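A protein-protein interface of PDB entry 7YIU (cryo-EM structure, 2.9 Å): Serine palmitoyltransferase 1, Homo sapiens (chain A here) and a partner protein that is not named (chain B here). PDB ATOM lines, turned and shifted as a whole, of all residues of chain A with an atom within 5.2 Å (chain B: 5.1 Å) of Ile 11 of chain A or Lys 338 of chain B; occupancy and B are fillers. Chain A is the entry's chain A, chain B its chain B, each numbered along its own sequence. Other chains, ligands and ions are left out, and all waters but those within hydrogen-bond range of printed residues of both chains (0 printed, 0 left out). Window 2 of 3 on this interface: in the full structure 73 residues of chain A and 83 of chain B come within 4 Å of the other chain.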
ATOM      1  N   LYS A   7     -14.808  29.060   0.466  1.00  0.00           N
ATOM      2  CA  LYS A   7     -15.766  28.260  -0.290  1.00  0.00           C
ATOM      3  C   LYS A   7     -15.179  26.954  -0.802  1.00  0.00           C
ATOM      4  O   LYS A   7     -15.797  25.907  -0.679  1.00  0.00           O
ATOM      5  CB  LYS A   7     -16.305  29.062  -1.474  1.00  0.00           C
ATOM      6  CG  LYS A   7     -17.693  29.633  -1.265  1.00  0.00           C
ATOM      7  CD  LYS A   7     -18.074  30.552  -2.410  1.00  0.00           C
ATOM      8  CE  LYS A   7     -19.473  31.108  -2.224  1.00  0.00           C
ATOM      9  NZ  LYS A   7     -19.731  32.249  -3.144  1.00  0.00           N
ATOM     10  N   GLU A   8     -13.982  27.019  -1.374  1.00  0.00           N
ATOM     11  CA  GLU A   8     -13.318  25.842  -1.919  1.00  0.00           C
ATOM     12  C   GLU A   8     -12.825  24.850  -0.867  1.00  0.00           C
ATOM     13  O   GLU A   8     -12.606  23.682  -1.171  1.00  0.00           O
ATOM     14  CB  GLU A   8     -12.154  26.265  -2.814  1.00  0.00           C
ATOM     15  CG  GLU A   8     -11.366  25.101  -3.385  1.00  0.00           C
ATOM     16  CD  GLU A   8     -12.221  24.188  -4.239  1.00  0.00           C
ATOM     17  OE1 GLU A   8     -12.054  24.204  -5.477  1.00  0.00           O
ATOM     18  OE2 GLU A   8     -13.060  23.454  -3.674  1.00  0.00           O
ATOM     19  N   GLU A   9     -12.633  25.315   0.362  1.00  0.00           N
ATOM     20  CA  GLU A   9     -12.171  24.448   1.437  1.00  0.00           C
ATOM     21  C   GLU A   9     -13.347  23.772   2.124  1.00  0.00           C
ATOM     22  O   GLU A   9     -13.191  22.743   2.771  1.00  0.00           O
ATOM     23  CB  GLU A   9     -11.356  25.243   2.453  1.00  0.00           C
ATOM     24  CG  GLU A   9     -10.003  25.696   1.935  1.00  0.00           C
ATOM     25  CD  GLU A   9      -8.855  25.166   2.768  1.00  0.00           C
ATOM     26  OE1 GLU A   9      -8.807  23.941   3.003  1.00  0.00           O
ATOM     27  OE2 GLU A   9      -8.000  25.975   3.188  1.00  0.00           O
ATOM     28  N   LEU A  10     -14.527  24.363   1.977  1.00  0.00           N
ATOM     29  CA  LEU A  10     -15.744  23.829   2.568  1.00  0.00           C
ATOM     30  C   LEU A  10     -16.188  22.582   1.823  1.00  0.00           C
ATOM     31  O   LEU A  10     -16.779  21.682   2.408  1.00  0.00           O
ATOM     32  CB  LEU A  10     -16.857  24.873   2.521  1.00  0.00           C
ATOM     33  CG  LEU A  10     -17.481  25.288   3.849  1.00  0.00           C
ATOM     34  CD1 LEU A  10     -16.444  25.234   4.954  1.00  0.00           C
ATOM     35  CD2 LEU A  10     -18.082  26.677   3.744  1.00  0.00           C
ATOM     36  N   ILE A  11     -15.892  22.535   0.529  1.00  0.00           N
ATOM     37  CA  ILE A  11     -16.255  21.402  -0.314  1.00  0.00           C
ATOM     38  C   ILE A  11     -15.284  20.233  -0.163  1.00  0.00           C
ATOM     39  O   ILE A  11     -15.576  19.119  -0.581  1.00  0.00           O
ATOM     40  CB  ILE A  11     -16.349  21.818  -1.796  1.00  0.00           C
ATOM     41  CG1 ILE A  11     -17.608  22.647  -2.034  1.00  0.00           C
ATOM     42  CG2 ILE A  11     -16.357  20.600  -2.702  1.00  0.00           C
ATOM     43  CD1 ILE A  11     -17.399  23.835  -2.943  1.00  0.00           C
ATOM     44  N   GLU A  12     -14.130  20.488   0.442  1.00  0.00           N
ATOM     45  CA  GLU A  12     -13.123  19.456   0.654  1.00  0.00           C
ATOM     46  C   GLU A  12     -13.298  18.769   2.001  1.00  0.00           C
ATOM     47  O   GLU A  12     -12.827  17.658   2.207  1.00  0.00           O
ATOM     48  CB  GLU A  12     -11.728  20.070   0.581  1.00  0.00           C
ATOM     49  CG  GLU A  12     -11.184  20.183  -0.827  1.00  0.00           C
ATOM     50  CD  GLU A  12     -11.450  18.936  -1.636  1.00  0.00           C
ATOM     51  OE1 GLU A  12     -10.512  18.132  -1.808  1.00  0.00           O
ATOM     52  OE2 GLU A  12     -12.599  18.759  -2.089  1.00  0.00           O
ATOM     53  N   GLU A  13     -13.973  19.450   2.917  1.00  0.00           N
ATOM     54  CA  GLU A  13     -14.217  18.938   4.257  1.00  0.00           C
ATOM     55  C   GLU A  13     -15.372  17.947   4.273  1.00  0.00           C
ATOM     56  O   GLU A  13     -15.353  16.978   5.036  1.00  0.00           O
ATOM     57  CB  GLU A  13     -14.516  20.090   5.218  1.00  0.00           C
ATOM     58  CG  GLU A  13     -13.299  20.774   5.809  1.00  0.00           C
ATOM     59  CD  GLU A  13     -13.679  21.910   6.746  1.00  0.00           C
ATOM     60  OE1 GLU A  13     -14.798  21.876   7.301  1.00  0.00           O
ATOM     61  OE2 GLU A  13     -12.866  22.840   6.921  1.00  0.00           O
ATOM     62  N   TRP A  14     -16.379  18.179   3.435  1.00  0.00           N
ATOM     63  CA  TRP A  14     -17.587  17.369   3.449  1.00  0.00           C
ATOM     64  C   TRP A  14     -17.276  15.921   3.112  1.00  0.00           C
ATOM     65  O   TRP A  14     -16.432  15.630   2.264  1.00  0.00           O
ATOM     66  CB  TRP A  14     -18.602  17.932   2.457  1.00  0.00           C
ATOM     67  CG  TRP A  14     -19.958  17.338   2.597  1.00  0.00           C
ATOM     68  CD1 TRP A  14     -20.775  17.415   3.680  1.00  0.00           C
ATOM     69  CD2 TRP A  14     -20.664  16.573   1.619  1.00  0.00           C
ATOM     70  NE1 TRP A  14     -21.942  16.743   3.442  1.00  0.00           N
ATOM     71  CE2 TRP A  14     -21.899  16.218   2.180  1.00  0.00           C
ATOM     72  CE3 TRP A  14     -20.371  16.152   0.323  1.00  0.00           C
ATOM     73  CZ2 TRP A  14     -22.837  15.465   1.494  1.00  0.00           C
ATOM     74  CZ3 TRP A  14     -21.304  15.411  -0.353  1.00  0.00           C
ATOM     75  CH2 TRP A  14     -22.520  15.071   0.231  1.00  0.00           C
ATOM     76  N   GLN A  15     -17.988  15.012   3.767  1.00  0.00           N
ATOM     77  CA  GLN A  15     -17.840  13.584   3.534  1.00  0.00           C
ATOM     78  C   GLN A  15     -19.210  12.965   3.733  1.00  0.00           C
ATOM     79  O   GLN A  15     -19.736  12.973   4.841  1.00  0.00           O
ATOM     80  CB  GLN A  15     -16.831  12.975   4.500  1.00  0.00           C
ATOM     81  CG  GLN A  15     -15.943  11.916   3.869  1.00  0.00           C
ATOM     82  CD  GLN A  15     -15.119  12.453   2.714  1.00  0.00           C
ATOM     83  OE1 GLN A  15     -14.225  13.275   2.901  1.00  0.00           O
ATOM     84  NE2 GLN A  15     -15.412  11.981   1.510  1.00  0.00           N
ATOM     85  N   PRO A  16     -19.801  12.423   2.661  1.00  0.00           N
ATOM     86  CA  PRO A  16     -21.148  11.868   2.786  1.00  0.00           C
ATOM     87  C   PRO A  16     -21.147  10.519   3.482  1.00  0.00           C
ATOM     88  O   PRO A  16     -20.114   9.872   3.655  1.00  0.00           O
ATOM     89  CB  PRO A  16     -21.601  11.733   1.332  1.00  0.00           C
ATOM     90  CG  PRO A  16     -20.336  11.522   0.592  1.00  0.00           C
ATOM     91  CD  PRO A  16     -19.327  12.390   1.268  1.00  0.00           C
ATOM     92  N   LYS B 293     -23.003  22.745  -6.056  1.00  0.00           N
ATOM     93  CA  LYS B 293     -22.011  23.526  -5.336  1.00  0.00           C
ATOM     94  C   LYS B 293     -22.580  24.258  -4.129  1.00  0.00           C
ATOM     95  O   LYS B 293     -22.066  24.124  -3.030  1.00  0.00           O
ATOM     96  CB  LYS B 293     -21.355  24.524  -6.284  1.00  0.00           C
ATOM     97  CG  LYS B 293     -20.157  25.241  -5.704  1.00  0.00           C
ATOM     98  CD  LYS B 293     -19.491  26.101  -6.759  1.00  0.00           C
ATOM     99  CE  LYS B 293     -18.630  25.260  -7.681  1.00  0.00           C
ATOM    100  NZ  LYS B 293     -17.265  25.064  -7.121  1.00  0.00           N
ATOM    101  N   ILE B 296     -23.576  22.278  -0.774  1.00  0.00           N
ATOM    102  CA  ILE B 296     -22.571  21.824   0.179  1.00  0.00           C
ATOM    103  C   ILE B 296     -22.084  22.941   1.087  1.00  0.00           C
ATOM    104  O   ILE B 296     -21.716  22.673   2.241  1.00  0.00           O
ATOM    105  CB  ILE B 296     -21.381  21.188  -0.566  1.00  0.00           C
ATOM    106  CG1 ILE B 296     -21.856  20.019  -1.423  1.00  0.00           C
ATOM    107  CG2 ILE B 296     -20.326  20.701   0.397  1.00  0.00           C
ATOM    108  CD1 ILE B 296     -20.733  19.230  -2.022  1.00  0.00           C
ATOM    109  N   VAL B 297     -22.039  24.163   0.570  1.00  0.00           N
ATOM    110  CA  VAL B 297     -21.555  25.296   1.347  1.00  0.00           C
ATOM    111  C   VAL B 297     -22.604  25.913   2.263  1.00  0.00           C
ATOM    112  O   VAL B 297     -22.272  26.418   3.330  1.00  0.00           O
ATOM    113  CB  VAL B 297     -20.948  26.395   0.447  1.00  0.00           C
ATOM    114  CG1 VAL B 297     -19.709  25.881  -0.258  1.00  0.00           C
ATOM    115  CG2 VAL B 297     -21.962  26.879  -0.569  1.00  0.00           C
ATOM    116  N   LYS B 334     -20.150  14.185 -10.490  1.00  0.00           N
ATOM    117  CA  LYS B 334     -20.531  13.500  -9.265  1.00  0.00           C
ATOM    118  C   LYS B 334     -19.311  12.891  -8.590  1.00  0.00           C
ATOM    119  O   LYS B 334     -19.390  12.402  -7.471  1.00  0.00           O
ATOM    120  CB  LYS B 334     -21.579  12.427  -9.548  1.00  0.00           C
ATOM    121  CG  LYS B 334     -21.029  11.203 -10.251  1.00  0.00           C
ATOM    122  CD  LYS B 334     -21.751   9.950  -9.802  1.00  0.00           C
ATOM    123  CE  LYS B 334     -20.868   9.107  -8.906  1.00  0.00           C
ATOM    124  NZ  LYS B 334     -20.628   7.759  -9.478  1.00  0.00           N
ATOM    125  N   LYS B 335     -18.180  12.915  -9.280  1.00  0.00           N
ATOM    126  CA  LYS B 335     -16.940  12.395  -8.732  1.00  0.00           C
ATOM    127  C   LYS B 335     -16.198  13.528  -8.039  1.00  0.00           C
ATOM    128  O   LYS B 335     -15.414  13.303  -7.123  1.00  0.00           O
ATOM    129  CB  LYS B 335     -16.068  11.812  -9.840  1.00  0.00           C
ATOM    130  CG  LYS B 335     -16.113  10.299  -9.931  1.00  0.00           C
ATOM    131  CD  LYS B 335     -15.696   9.819 -11.309  1.00  0.00           C
ATOM    132  CE  LYS B 335     -15.993   8.342 -11.489  1.00  0.00           C
ATOM    133  NZ  LYS B 335     -15.224   7.756 -12.618  1.00  0.00           N
ATOM    134  N   LYS B 336     -16.466  14.749  -8.482  1.00  0.00           N
ATOM    135  CA  LYS B 336     -15.826  15.930  -7.925  1.00  0.00           C
ATOM    136  C   LYS B 336     -16.568  16.492  -6.718  1.00  0.00           C
ATOM    137  O   LYS B 336     -16.013  17.288  -5.971  1.00  0.00           O
ATOM    138  CB  LYS B 336     -15.684  17.002  -9.001  1.00  0.00           C
ATOM    139  CG  LYS B 336     -15.505  18.405  -8.456  1.00  0.00           C
ATOM    140  CD  LYS B 336     -14.607  19.228  -9.360  1.00  0.00           C
ATOM    141  CE  LYS B 336     -15.416  20.182 -10.218  1.00  0.00           C
ATOM    142  NZ  LYS B 336     -14.538  21.123 -10.966  1.00  0.00           N
ATOM    143  N   TYR B 337     -17.819  16.083  -6.532  1.00  0.00           N
ATOM    144  CA  TYR B 337     -18.621  16.548  -5.404  1.00  0.00           C
ATOM    145  C   TYR B 337     -19.129  15.388  -4.558  1.00  0.00           C
ATOM    146  O   TYR B 337     -19.985  15.562  -3.698  1.00  0.00           O
ATOM    147  CB  TYR B 337     -19.794  17.401  -5.879  1.00  0.00           C
ATOM    148  CG  TYR B 337     -19.383  18.718  -6.483  1.00  0.00           C
ATOM    149  CD1 TYR B 337     -18.969  19.768  -5.684  1.00  0.00           C
ATOM    150  CD2 TYR B 337     -19.403  18.908  -7.851  1.00  0.00           C
ATOM    151  CE1 TYR B 337     -18.588  20.972  -6.234  1.00  0.00           C
ATOM    152  CE2 TYR B 337     -19.025  20.108  -8.407  1.00  0.00           C
ATOM    153  CZ  TYR B 337     -18.620  21.134  -7.594  1.00  0.00           C
ATOM    154  OH  TYR B 337     -18.243  22.331  -8.148  1.00  0.00           O
ATOM    155  N   LYS B 338     -18.604  14.202  -4.826  1.00  0.00           N
ATOM    156  CA  LYS B 338     -18.958  12.998  -4.087  1.00  0.00           C
ATOM    157  C   LYS B 338     -20.451  12.704  -3.941  1.00  0.00           C
ATOM    158  O   LYS B 338     -20.893  12.255  -2.889  1.00  0.00           O
ATOM    159  CB  LYS B 338     -18.286  13.015  -2.714  1.00  0.00           C
ATOM    160  CG  LYS B 338     -16.794  13.290  -2.768  1.00  0.00           C
ATOM    161  CD  LYS B 338     -16.277  13.801  -1.438  1.00  0.00           C
ATOM    162  CE  LYS B 338     -16.357  15.314  -1.361  1.00  0.00           C
ATOM    163  NZ  LYS B 338     -15.339  15.869  -0.430  1.00  0.00           N
ATOM    164  N   ALA B 339     -21.219  12.929  -5.000  1.00  0.00           N
ATOM    165  CA  ALA B 339     -22.649  12.653  -4.978  1.00  0.00           C
ATOM    166  C   ALA B 339     -22.895  11.240  -5.484  1.00  0.00           C
ATOM    167  O   ALA B 339     -21.967  10.562  -5.911  1.00  0.00           O
ATOM    168  CB  ALA B 339     -23.394  13.659  -5.830  1.00  0.00           C
ATOM    169  N   TYR B 340     -24.142  10.788  -5.427  1.00  0.00           N
ATOM    170  CA  TYR B 340     -24.487   9.454  -5.895  1.00  0.00           C
ATOM    171  C   TYR B 340     -25.337   9.566  -7.150  1.00  0.00           C
ATOM    172  O   TYR B 340     -26.017  10.561  -7.349  1.00  0.00           O
ATOM    173  CB  TYR B 340     -25.209   8.669  -4.803  1.00  0.00           C
ATOM    174  CG  TYR B 340     -24.332   8.393  -3.608  1.00  0.00           C
ATOM    175  CD1 TYR B 340     -23.129   7.725  -3.749  1.00  0.00           C
ATOM    176  CD2 TYR B 340     -24.697   8.815  -2.342  1.00  0.00           C
ATOM    177  CE1 TYR B 340     -22.320   7.479  -2.663  1.00  0.00           C
ATOM    178  CE2 TYR B 340     -23.891   8.572  -1.250  1.00  0.00           C
ATOM    179  CZ  TYR B 340     -22.704   7.904  -1.420  1.00  0.00           C
ATOM    180  OH  TYR B 340     -21.897   7.658  -0.341  1.00  0.00           O
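O of Lys 7 of chain A touches CG1 of Val 297 of chain B (3.9 Å).
CG2 of Ile 296 of chain B touches CB of Trp 14 of chain A, 3.9 Å away.
Trp 14 of chain A touches Tyr 337 of chain B.
Lys 338 of chain B touches Gln 15 of chain A (CD to NE2, 3.6 Å).
Lys 338 of chain B touches Pro 16 of chain A.
The side-chain amino group (NZ) of Lys 293 of chain B lies close to the side-chain hydroxyl (OH) of Tyr 337 of chain B (3.1 Å).
Of the 10 printed residues of chain B, 4 touch a printed residue of chain A.
Along chain A the printed residues that touch a printed residue of chain B span positions 7 to 16.
Among the printed residues, 7 pairs touch across the chains.
Among the printed residues, no Asp or Glu carboxylate lies within 4 Å of a Lys or Arg side-chain nitrogen of the other chain.
Lys 338 of chain B touches four residues of chain A.
Of the printed residues of chain B, Trp 14 of chain A touches Ile 296, Tyr 337 and Lys 338.
Printed residues of chain B within 4 Å of Lys 7 of chain A: Val 297.
Of the printed residues of chain B, Gln 15 of chain A touches Lys 338 (3.6 Å).
The nearest residue of chain B that does not touch Ile 11 of chain A is Tyr 337 of chain B (4.1 Å).
The nearest residue of chain A that does not touch Lys 338 of chain B is Glu 12 of chain A (4.1 Å).
The nearest printed residue of chain A that does not touch Val 297 of chain B is Ile 11 of chain A (4.1 Å).
The side-chain amino group (NZ) of Lys 338 of chain B lies within hydrogen-bond range of the backbone carbonyl oxygen (O) of Ile 11 of chain A.
O of Trp 14 of chain A lies within hydrogen-bond range of NZ of Lys 338 of chain B (2.9 Å).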
